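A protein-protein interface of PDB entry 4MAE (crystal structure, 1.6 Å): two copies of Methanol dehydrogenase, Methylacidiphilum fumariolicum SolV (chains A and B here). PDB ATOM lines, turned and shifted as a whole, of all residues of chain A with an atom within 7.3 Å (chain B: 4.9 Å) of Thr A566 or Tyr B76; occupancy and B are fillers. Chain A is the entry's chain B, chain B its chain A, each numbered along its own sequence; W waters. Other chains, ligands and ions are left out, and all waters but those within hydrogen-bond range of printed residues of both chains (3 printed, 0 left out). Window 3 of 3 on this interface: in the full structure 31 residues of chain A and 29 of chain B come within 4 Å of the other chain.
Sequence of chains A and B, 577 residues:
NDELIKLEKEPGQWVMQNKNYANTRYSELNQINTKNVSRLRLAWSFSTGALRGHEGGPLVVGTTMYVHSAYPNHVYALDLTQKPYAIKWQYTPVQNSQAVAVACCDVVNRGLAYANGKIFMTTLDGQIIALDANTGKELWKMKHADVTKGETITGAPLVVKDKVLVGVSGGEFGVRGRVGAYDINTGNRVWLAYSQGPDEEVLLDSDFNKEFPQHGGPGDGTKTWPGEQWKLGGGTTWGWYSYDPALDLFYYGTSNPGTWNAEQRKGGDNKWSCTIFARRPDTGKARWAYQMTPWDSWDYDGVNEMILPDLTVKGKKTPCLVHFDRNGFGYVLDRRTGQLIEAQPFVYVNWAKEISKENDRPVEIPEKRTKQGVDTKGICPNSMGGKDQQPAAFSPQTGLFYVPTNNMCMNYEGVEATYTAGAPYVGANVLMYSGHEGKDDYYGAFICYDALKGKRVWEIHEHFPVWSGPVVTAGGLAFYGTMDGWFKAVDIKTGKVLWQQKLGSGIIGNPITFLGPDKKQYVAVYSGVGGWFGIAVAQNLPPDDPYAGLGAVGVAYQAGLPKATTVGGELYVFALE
Water W1 lies within hydrogen-bond range of the backbone carbonyl oxygen of Thr A565 (2.7 Å), the backbone carbonyl oxygen of Pro A562 (3.0 Å) and the side-chain amide nitrogen of Gln B90 (3.4 Å).
Water W3 bridges the backbone NH (N) of Ile B87 (2.8 Å) and the backbone carbonyl oxygen (O) of Lys A563 (3.0 Å).
Water W2 lies within hydrogen-bond range of O of Ile B87 and O of Lys A563.
CA of Gly A504 touches CA of Phe B46, 3.6 Å away.
O of Pro A562 touches NE2 of Gln B90, 3.7 Å away.
Ile B87 touches Lys A563.
Ala A564 touches Ile B87 (C to CD1, 3.9 Å).
Ile B87 touches Thr A565.
Thr A566 touches Phe B46 (CG2 to CZ, 3.9 Å).
Thr A566 touches Tyr B76 (CG2 to CE1, 3.5 Å).
Gly B49 touches Val A567 (CA to O, 3.4 Å).
Ser B47 touches Gly A568 (OG to CA, 3.5 Å).
Val A537 touches none of the printed residues of chain B.
Printed residues of chain B within 4 Å of Lys A563: Ile B87.
Thr A566 touches just these residues of chain B: Phe B46 (3.9 Å), Ser B47 (2.7 Å) and Tyr B76 (3.5 Å).
Of the printed residues of chain B, Gly A568 touches Ser B47.
Printed residues of chain A within 4 Å of Phe B46: Gly A504 (3.6 Å) and Thr A566 (3.9 Å).
Printed residues of chain A within 4 Å of Ser B47: Gly A504, Thr A566, Val A567 and Gly A568.
Of chain A, only Thr A566 comes within 4 Å of Tyr B76.
Of the printed residues of chain A, Ile B87 touches Lys A563 (3.6 Å), Ala A564 (3.9 Å) and Thr A565 (3.9 Å).
The nearest residue of chain A that does not touch Tyr B76 is Val A567 (6.1 Å).
The nearest printed residue of chain B that does not touch Ala A564 is Gln B90 (6.3 Å).
No position is printed for both chains.
Of the 12 pairs that touch across the chains among the printed residues, none has its exchanged pair printed and touching as well.
O of Ser B47 lies within hydrogen-bond range of OG1 of Thr A566, 2.7 Å away.
The side-chain hydroxyl (OG) of Ser B47 lies within hydrogen-bond range of the backbone carbonyl oxygen (O) of Val A567, 2.6 Å away.
N of Ser B47 sits at hydrogen-bond distance from O of Gly A504.
The backbone carbonyl oxygen (O) of Thr B48 is in hydrogen-bond range of the side-chain hydroxyl (OH) of Tyr B76, 2.6 Å away.
The backbone carbonyl oxygen (O) of Thr A566 sits at hydrogen-bond distance from the side-chain hydroxyl (OG) of Ser A505 (2.6 Å).
N of Val B67 is in hydrogen-bond range of O of Tyr B76 (2.9 Å).
N of Gly A506 sits at hydrogen-bond distance from OG1 of Thr A565, 2.9 Å away.
The backbone NH (N) of Gly B49 lies close to the side-chain hydroxyl (OG) of Ser B47, at 3.4 Å.
Printed residues of chain B that touch a printed residue of chain A: Phe B46, Ser B47, Gly B49, Tyr B76, Ile B87 and Gln B90.
Hydrophobic or aromatic side chains of chain B that line the printed part of chain A: Phe B46, Tyr B76 and Ile B87.
Of the 19 printed residues of chain A, 8 touch a printed residue of chain B.
Hydrophobic or aromatic side chains of chain A within 4 Å of the printed part of chain B: Val A567.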
ATOM      1  N   MET A 483      31.401 -18.011  14.427  1.00  0.00           N
ATOM      2  CA  MET A 483      31.997 -17.707  13.126  1.00  0.00           C
ATOM      3  C   MET A 483      31.556 -18.656  12.009  1.00  0.00           C
ATOM      4  O   MET A 483      31.894 -18.437  10.835  1.00  0.00           O
ATOM      5  CB  MET A 483      33.526 -17.675  13.241  1.00  0.00           C
ATOM      6  CG  MET A 483      34.028 -16.571  14.158  1.00  0.00           C
ATOM      7  SD  MET A 483      35.766 -16.161  13.863  1.00  0.00           S
ATOM      8  CE  MET A 483      35.680 -15.407  12.239  1.00  0.00           C
ATOM      9  N   GLY A 504      23.154 -17.050   7.763  1.00  0.00           N
ATOM     10  CA  GLY A 504      23.752 -17.220   6.443  1.00  0.00           C
ATOM     11  C   GLY A 504      25.266 -17.129   6.331  1.00  0.00           C
ATOM     12  O   GLY A 504      25.850 -17.659   5.375  1.00  0.00           O
ATOM     13  N   SER A 505      25.894 -16.455   7.291  1.00  0.00           N
ATOM     14  CA  SER A 505      27.335 -16.240   7.296  1.00  0.00           C
ATOM     15  C   SER A 505      27.811 -16.133   8.739  1.00  0.00           C
ATOM     16  O   SER A 505      27.041 -15.767   9.627  1.00  0.00           O
ATOM     17  CB  SER A 505      27.680 -14.950   6.536  1.00  0.00           C
ATOM     18  OG  SER A 505      29.080 -14.760   6.419  1.00  0.00           O
ATOM     19  N   GLY A 506      29.083 -16.439   8.966  1.00  0.00           N
ATOM     20  CA  GLY A 506      29.700 -16.229  10.267  1.00  0.00           C
ATOM     21  C   GLY A 506      29.359 -14.869  10.850  1.00  0.00           C
ATOM     22  O   GLY A 506      29.293 -13.878  10.136  1.00  0.00           O
ATOM     23  N   SER A 527      25.195 -10.523  10.336  1.00  0.00           N
ATOM     24  CA  SER A 527      25.859 -11.716   9.839  1.00  0.00           C
ATOM     25  C   SER A 527      26.721 -11.300   8.634  1.00  0.00           C
ATOM     26  O   SER A 527      26.343 -10.415   7.853  1.00  0.00           O
ATOM     27  CB  SER A 527      24.791 -12.763   9.475  1.00  0.00           C
ATOM     28  OG  SER A 527      25.257 -13.733   8.570  1.00  0.00           O
ATOM     29  N   GLY A 528      27.883 -11.923   8.481  1.00  0.00           N
ATOM     30  CA  GLY A 528      28.853 -11.496   7.477  1.00  0.00           C
ATOM     31  C   GLY A 528      30.254 -11.642   8.028  1.00  0.00           C
ATOM     32  O   GLY A 528      30.756 -10.767   8.737  1.00  0.00           O
ATOM     33  N   VAL A 529      30.874 -12.776   7.719  1.00  0.00           N
ATOM     34  CA  VAL A 529      32.120 -13.168   8.348  1.00  0.00           C
ATOM     35  C   VAL A 529      33.285 -12.339   7.798  1.00  0.00           C
ATOM     36  O   VAL A 529      33.242 -11.842   6.672  1.00  0.00           O
ATOM     37  CB  VAL A 529      32.360 -14.708   8.192  1.00  0.00           C
ATOM     38  CG1 VAL A 529      32.887 -15.046   6.802  1.00  0.00           C
ATOM     39  CG2 VAL A 529      33.291 -15.240   9.286  1.00  0.00           C
ATOM     40  N   GLY A 530      34.312 -12.179   8.617  1.00  0.00           N
ATOM     41  CA  GLY A 530      35.501 -11.437   8.225  1.00  0.00           C
ATOM     42  C   GLY A 530      36.329 -11.114   9.446  1.00  0.00           C
ATOM     43  O   GLY A 530      36.407 -11.913  10.384  1.00  0.00           O
ATOM     44  N   VAL A 537      38.661 -16.111   4.400  1.00  0.00           N
ATOM     45  CA  VAL A 537      37.357 -16.152   3.750  1.00  0.00           C
ATOM     46  C   VAL A 537      36.999 -14.794   3.149  1.00  0.00           C
ATOM     47  O   VAL A 537      36.644 -14.721   1.976  1.00  0.00           O
ATOM     48  CB  VAL A 537      36.266 -16.630   4.718  1.00  0.00           C
ATOM     49  CG1 VAL A 537      34.904 -16.642   4.032  1.00  0.00           C
ATOM     50  CG2 VAL A 537      36.608 -18.011   5.244  1.00  0.00           C
ATOM     51  N   ALA A 538      37.099 -13.724   3.933  1.00  0.00           N
ATOM     52  CA  ALA A 538      36.733 -12.390   3.442  1.00  0.00           C
ATOM     53  C   ALA A 538      37.545 -11.974   2.215  1.00  0.00           C
ATOM     54  O   ALA A 538      37.004 -11.368   1.286  1.00  0.00           O
ATOM     55  CB  ALA A 538      36.865 -11.346   4.561  1.00  0.00           C
ATOM     56  N   LEU A 561      37.589 -22.990   8.811  1.00  0.00           N
ATOM     57  CA  LEU A 561      36.657 -21.878   8.585  1.00  0.00           C
ATOM     58  C   LEU A 561      36.213 -21.767   7.122  1.00  0.00           C
ATOM     59  O   LEU A 561      35.027 -21.575   6.862  1.00  0.00           O
ATOM     60  CB  LEU A 561      37.239 -20.547   9.065  1.00  0.00           C
ATOM     61  CG  LEU A 561      36.256 -19.380   9.114  1.00  0.00           C
ATOM     62  CD1 LEU A 561      35.218 -19.601  10.214  1.00  0.00           C
ATOM     63  CD2 LEU A 561      37.002 -18.091   9.339  1.00  0.00           C
ATOM     64  N   PRO A 562      37.152 -21.888   6.163  1.00  0.00           N
ATOM     65  CA  PRO A 562      36.732 -21.780   4.763  1.00  0.00           C
ATOM     66  C   PRO A 562      35.716 -22.840   4.338  1.00  0.00           C
ATOM     67  O   PRO A 562      34.947 -22.611   3.407  1.00  0.00           O
ATOM     68  CB  PRO A 562      38.053 -21.916   3.998  1.00  0.00           C
ATOM     69  CG  PRO A 562      39.060 -21.348   4.946  1.00  0.00           C
ATOM     70  CD  PRO A 562      38.624 -21.878   6.279  1.00  0.00           C
ATOM     71  N   LYS A 563      35.704 -23.980   5.022  1.00  0.00           N
ATOM     72  CA  LYS A 563      34.707 -25.028   4.778  1.00  0.00           C
ATOM     73  C   LYS A 563      33.399 -24.802   5.536  1.00  0.00           C
ATOM     74  O   LYS A 563      32.430 -25.546   5.339  1.00  0.00           O
ATOM     75  CB  LYS A 563      35.268 -26.394   5.184  1.00  0.00           C
ATOM     76  CG  LYS A 563      36.370 -26.904   4.279  1.00  0.00           C
ATOM     77  CD  LYS A 563      37.014 -28.191   4.819  1.00  0.00           C
ATOM     78  CE  LYS A 563      35.993 -29.316   5.017  1.00  0.00           C
ATOM     79  NZ  LYS A 563      36.633 -30.681   5.034  1.00  0.00           N
ATOM     80  N   ALA A 564      33.369 -23.808   6.421  1.00  0.00           N
ATOM     81  CA  ALA A 564      32.241 -23.634   7.338  1.00  0.00           C
ATOM     82  C   ALA A 564      31.342 -22.444   7.015  1.00  0.00           C
ATOM     83  O   ALA A 564      30.206 -22.396   7.494  1.00  0.00           O
ATOM     84  CB  ALA A 564      32.752 -23.505   8.755  1.00  0.00           C
ATOM     85  N   THR A 565      31.840 -21.481   6.241  1.00  0.00           N
ATOM     86  CA  THR A 565      31.112 -20.234   6.042  1.00  0.00           C
ATOM     87  C   THR A 565      31.474 -19.542   4.732  1.00  0.00           C
ATOM     88  O   THR A 565      32.620 -19.587   4.273  1.00  0.00           O
ATOM     89  CB  THR A 565      31.357 -19.246   7.221  1.00  0.00           C
ATOM     90  OG1 THR A 565      30.562 -18.057   7.057  1.00  0.00           O
ATOM     91  CG2 THR A 565      32.826 -18.858   7.309  1.00  0.00           C
ATOM     92  N   THR A 566      30.472 -18.894   4.147  1.00  0.00           N
ATOM     93  CA  THR A 566      30.653 -17.993   3.026  1.00  0.00           C
ATOM     94  C   THR A 566      30.628 -16.551   3.534  1.00  0.00           C
ATOM     95  O   THR A 566      30.332 -16.292   4.712  1.00  0.00           O
ATOM     96  CB  THR A 566      29.514 -18.160   2.011  1.00  0.00           C
ATOM     97  OG1 THR A 566      28.266 -17.997   2.696  1.00  0.00           O
ATOM     98  CG2 THR A 566      29.571 -19.531   1.356  1.00  0.00           C
ATOM     99  N   VAL A 567      30.944 -15.617   2.646  1.00  0.00           N
ATOM    100  CA  VAL A 567      30.804 -14.198   2.957  1.00  0.00           C
ATOM    101  C   VAL A 567      29.360 -13.741   2.828  1.00  0.00           C
ATOM    102  O   VAL A 567      28.527 -14.373   2.151  1.00  0.00           O
ATOM    103  CB  VAL A 567      31.710 -13.295   2.089  1.00  0.00           C
ATOM    104  CG1 VAL A 567      33.177 -13.629   2.331  1.00  0.00           C
ATOM    105  CG2 VAL A 567      31.353 -13.410   0.601  1.00  0.00           C
ATOM    106  N   GLY A 568      29.077 -12.621   3.478  1.00  0.00           N
ATOM    107  CA  GLY A 568      27.747 -12.063   3.493  1.00  0.00           C
ATOM    108  C   GLY A 568      27.704 -10.685   4.119  1.00  0.00           C
ATOM    109  O   GLY A 568      28.744 -10.062   4.377  1.00  0.00           O
ATOM    110  N   GLY A 569      26.485 -10.212   4.347  1.00  0.00           N
ATOM    111  CA  GLY A 569      26.253  -8.906   4.951  1.00  0.00           C
ATOM    112  C   GLY A 569      24.767  -8.697   5.103  1.00  0.00           C
ATOM    113  O   GLY A 569      24.134  -8.112   4.233  1.00  0.00           O
ATOM    114  N   PHE B  46      21.395 -19.228   4.441  1.00  0.00           N
ATOM    115  CA  PHE B  46      22.713 -19.466   3.866  1.00  0.00           C
ATOM    116  C   PHE B  46      23.034 -18.356   2.867  1.00  0.00           C
ATOM    117  O   PHE B  46      22.254 -18.119   1.953  1.00  0.00           O
ATOM    118  CB  PHE B  46      22.722 -20.827   3.161  1.00  0.00           C
ATOM    119  CG  PHE B  46      23.977 -21.101   2.388  1.00  0.00           C
ATOM    120  CD1 PHE B  46      25.166 -21.363   3.054  1.00  0.00           C
ATOM    121  CD2 PHE B  46      23.974 -21.099   0.999  1.00  0.00           C
ATOM    122  CE1 PHE B  46      26.323 -21.613   2.351  1.00  0.00           C
ATOM    123  CE2 PHE B  46      25.135 -21.354   0.290  1.00  0.00           C
ATOM    124  CZ  PHE B  46      26.309 -21.608   0.971  1.00  0.00           C
ATOM    125  N   SER B  47      24.169 -17.677   3.052  1.00  0.00           N
ATOM    126  CA  SER B  47      24.603 -16.623   2.134  1.00  0.00           C
ATOM    127  C   SER B  47      25.298 -17.211   0.906  1.00  0.00           C
ATOM    128  O   SER B  47      26.187 -18.059   1.028  1.00  0.00           O
ATOM    129  CB  SER B  47      25.557 -15.645   2.838  1.00  0.00           C
ATOM    130  OG  SER B  47      25.917 -14.593   1.964  1.00  0.00           O
ATOM    131  N   THR B  48      24.911 -16.746  -0.276  1.00  0.00           N
ATOM    132  CA  THR B  48      25.527 -17.213  -1.520  1.00  0.00           C
ATOM    133  C   THR B  48      26.895 -16.575  -1.781  1.00  0.00           C
ATOM    134  O   THR B  48      27.639 -17.024  -2.658  1.00  0.00           O
ATOM    135  CB  THR B  48      24.624 -16.912  -2.734  1.00  0.00           C
ATOM    136  OG1 THR B  48      24.487 -15.494  -2.874  1.00  0.00           O
ATOM    137  CG2 THR B  48      23.252 -17.550  -2.569  1.00  0.00           C
ATOM    138  N   GLY B  49      27.220 -15.517  -1.037  1.00  0.00           N
ATOM    139  CA  GLY B  49      28.493 -14.837  -1.196  1.00  0.00           C
ATOM    140  C   GLY B  49      28.553 -13.949  -2.423  1.00  0.00           C
ATOM    141  O   GLY B  49      29.638 -13.523  -2.825  1.00  0.00           O
ATOM    142  N   MET B  65      21.153 -30.210  -0.862  1.00  0.00           N
ATOM    143  CA  MET B  65      20.633 -29.031  -1.549  1.00  0.00           C
ATOM    144  C   MET B  65      21.743 -28.404  -2.374  1.00  0.00           C
ATOM    145  O   MET B  65      22.871 -28.256  -1.896  1.00  0.00           O
ATOM    146  CB  MET B  65      20.102 -27.988  -0.569  1.00  0.00           C
ATOM    147  CG  MET B  65      19.473 -26.790  -1.278  1.00  0.00           C
ATOM    148  SD  MET B  65      18.847 -25.510  -0.199  1.00  0.00           S
ATOM    149  CE  MET B  65      17.405 -26.314   0.520  1.00  0.00           C
ATOM    150  N   TYR B  66      21.418 -28.032  -3.606  1.00  0.00           N
ATOM    151  CA  TYR B  66      22.370 -27.387  -4.500  1.00  0.00           C
ATOM    152  C   TYR B  66      21.954 -25.935  -4.711  1.00  0.00           C
ATOM    153  O   TYR B  66      20.805 -25.652  -5.059  1.00  0.00           O
ATOM    154  CB  TYR B  66      22.442 -28.154  -5.821  1.00  0.00           C
ATOM    155  CG  TYR B  66      22.922 -29.564  -5.623  1.00  0.00           C
ATOM    156  CD1 TYR B  66      22.020 -30.605  -5.458  1.00  0.00           C
ATOM    157  CD2 TYR B  66      24.282 -29.855  -5.550  1.00  0.00           C
ATOM    158  CE1 TYR B  66      22.460 -31.903  -5.254  1.00  0.00           C
ATOM    159  CE2 TYR B  66      24.731 -31.152  -5.343  1.00  0.00           C
ATOM    160  CZ  TYR B  66      23.815 -32.174  -5.200  1.00  0.00           C
ATOM    161  OH  TYR B  66      24.231 -33.482  -4.993  1.00  0.00           O
ATOM    162  N   VAL B  67      22.896 -25.032  -4.479  1.00  0.00           N
ATOM    163  CA  VAL B  67      22.639 -23.611  -4.434  1.00  0.00           C
ATOM    164  C   VAL B  67      23.532 -22.931  -5.463  1.00  0.00           C
ATOM    165  O   VAL B  67      24.671 -23.349  -5.672  1.00  0.00           O
ATOM    166  CB  VAL B  67      22.955 -23.067  -3.033  1.00  0.00           C
ATOM    167  CG1 VAL B  67      22.778 -21.547  -2.967  1.00  0.00           C
ATOM    168  CG2 VAL B  67      22.097 -23.778  -1.982  1.00  0.00           C
ATOM    169  N   HIS B  74      28.965 -18.812  -8.110  1.00  0.00           N
ATOM    170  CA  HIS B  74      29.366 -19.772  -7.082  1.00  0.00           C
ATOM    171  C   HIS B  74      28.324 -20.872  -7.033  1.00  0.00           C
ATOM    172  O   HIS B  74      27.142 -20.595  -7.184  1.00  0.00           O
ATOM    173  CB  HIS B  74      29.425 -19.120  -5.703  1.00  0.00           C
ATOM    174  CG  HIS B  74      30.295 -17.905  -5.635  1.00  0.00           C
ATOM    175  ND1 HIS B  74      31.652 -17.951  -5.855  1.00  0.00           N
ATOM    176  CD2 HIS B  74      30.005 -16.617  -5.337  1.00  0.00           C
ATOM    177  CE1 HIS B  74      32.159 -16.737  -5.724  1.00  0.00           C
ATOM    178  NE2 HIS B  74      31.180 -15.910  -5.402  1.00  0.00           N
ATOM    179  N   VAL B  75      28.765 -22.105  -6.811  1.00  0.00           N
ATOM    180  CA  VAL B  75      27.861 -23.252  -6.650  1.00  0.00           C
ATOM    181  C   VAL B  75      28.221 -23.979  -5.362  1.00  0.00           C
ATOM    182  O   VAL B  75      29.401 -24.188  -5.064  1.00  0.00           O
ATOM    183  CB  VAL B  75      27.948 -24.223  -7.856  1.00  0.00           C
ATOM    184  CG1 VAL B  75      27.179 -25.516  -7.588  1.00  0.00           C
ATOM    185  CG2 VAL B  75      27.426 -23.548  -9.111  1.00  0.00           C
ATOM    186  N   TYR B  76      27.198 -24.337  -4.588  1.00  0.00           N
ATOM    187  CA  TYR B  76      27.387 -24.968  -3.298  1.00  0.00           C
ATOM    188  C   TYR B  76      26.504 -26.198  -3.201  1.00  0.00           C
ATOM    189  O   TYR B  76      25.385 -26.203  -3.702  1.00  0.00           O
ATOM    190  CB  TYR B  76      26.987 -24.022  -2.168  1.00  0.00           C
ATOM    191  CG  TYR B  76      27.635 -22.667  -2.206  1.00  0.00           C
ATOM    192  CD1 TYR B  76      28.893 -22.459  -1.650  1.00  0.00           C
ATOM    193  CD2 TYR B  76      26.994 -21.588  -2.799  1.00  0.00           C
ATOM    194  CE1 TYR B  76      29.495 -21.213  -1.686  1.00  0.00           C
ATOM    195  CE2 TYR B  76      27.581 -20.342  -2.839  1.00  0.00           C
ATOM    196  CZ  TYR B  76      28.831 -20.157  -2.272  1.00  0.00           C
ATOM    197  OH  TYR B  76      29.419 -18.909  -2.303  1.00  0.00           O
ATOM    198  N   ALA B  77      27.031 -27.235  -2.563  1.00  0.00           N
ATOM    199  CA  ALA B  77      26.251 -28.391  -2.166  1.00  0.00           C
ATOM    200  C   ALA B  77      26.144 -28.353  -0.645  1.00  0.00           C
ATOM    201  O   ALA B  77      27.162 -28.270   0.063  1.00  0.00           O
ATOM    202  CB  ALA B  77      26.922 -29.683  -2.622  1.00  0.00           C
ATOM    203  N   LEU B  78      24.910 -28.395  -0.150  1.00  0.00           N
ATOM    204  CA  LEU B  78      24.641 -28.381   1.287  1.00  0.00           C
ATOM    205  C   LEU B  78      24.126 -29.745   1.759  1.00  0.00           C
ATOM    206  O   LEU B  78      23.159 -30.278   1.204  1.00  0.00           O
ATOM    207  CB  LEU B  78      23.621 -27.292   1.630  1.00  0.00           C
ATOM    208  CG  LEU B  78      23.901 -25.848   1.197  1.00  0.00           C
ATOM    209  CD1 LEU B  78      22.801 -24.927   1.712  1.00  0.00           C
ATOM    210  CD2 LEU B  78      25.284 -25.361   1.663  1.00  0.00           C
ATOM    211  N   ILE B  87      28.184 -27.206   4.674  1.00  0.00           N
ATOM    212  CA  ILE B  87      28.649 -27.051   3.302  1.00  0.00           C
ATOM    213  C   ILE B  87      29.433 -28.296   2.909  1.00  0.00           C
ATOM    214  O   ILE B  87      30.504 -28.556   3.455  1.00  0.00           O
ATOM    215  CB  ILE B  87      29.540 -25.795   3.140  1.00  0.00           C
ATOM    216  CG1 ILE B  87      28.787 -24.537   3.587  1.00  0.00           C
ATOM    217  CG2 ILE B  87      29.982 -25.645   1.697  1.00  0.00           C
ATOM    218  CD1 ILE B  87      29.648 -23.261   3.572  1.00  0.00           C
ATOM    219  N   TRP B  89      30.411 -29.204  -0.425  1.00  0.00           N
ATOM    220  CA  TRP B  89      31.450 -28.747  -1.331  1.00  0.00           C
ATOM    221  C   TRP B  89      31.062 -27.425  -1.957  1.00  0.00           C
ATOM    222  O   TRP B  89      29.905 -27.018  -1.901  1.00  0.00           O
ATOM    223  CB  TRP B  89      31.768 -29.800  -2.405  1.00  0.00           C
ATOM    224  CG  TRP B  89      30.622 -30.286  -3.298  1.00  0.00           C
ATOM    225  CD1 TRP B  89      29.949 -31.475  -3.188  1.00  0.00           C
ATOM    226  CD2 TRP B  89      30.071 -29.627  -4.459  1.00  0.00           C
ATOM    227  NE1 TRP B  89      29.019 -31.592  -4.193  1.00  0.00           N
ATOM    228  CE2 TRP B  89      29.067 -30.472  -4.983  1.00  0.00           C
ATOM    229  CE3 TRP B  89      30.322 -28.408  -5.099  1.00  0.00           C
ATOM    230  CZ2 TRP B  89      28.321 -30.138  -6.120  1.00  0.00           C
ATOM    231  CZ3 TRP B  89      29.570 -28.072  -6.225  1.00  0.00           C
ATOM    232  CH2 TRP B  89      28.578 -28.937  -6.720  1.00  0.00           C
ATOM    233  N   GLN B  90      32.046 -26.729  -2.516  1.00  0.00           N
ATOM    234  CA  GLN B  90      31.762 -25.550  -3.302  1.00  0.00           C
ATOM    235  C   GLN B  90      32.633 -25.463  -4.536  1.00  0.00           C
ATOM    236  O   GLN B  90      33.746 -26.006  -4.576  1.00  0.00           O
ATOM    237  CB  GLN B  90      31.892 -24.280  -2.471  1.00  0.00           C
ATOM    238  CG  GLN B  90      33.224 -24.034  -1.862  1.00  0.00           C
ATOM    239  CD  GLN B  90      33.259 -22.706  -1.137  1.00  0.00           C
ATOM    240  OE1 GLN B  90      33.457 -21.653  -1.755  1.00  0.00           O
ATOM    241  NE2 GLN B  90      33.052 -22.742   0.181  1.00  0.00           N
HETATM  242  O   HOH W   1      34.092 -20.112   2.065  1.00  0.00           O
HETATM  243  O   HOH W   2      31.912 -28.886   6.020  1.00  0.00           O
HETATM  244  O   HOH W   3      29.868 -26.243   6.743  1.00  0.00           O
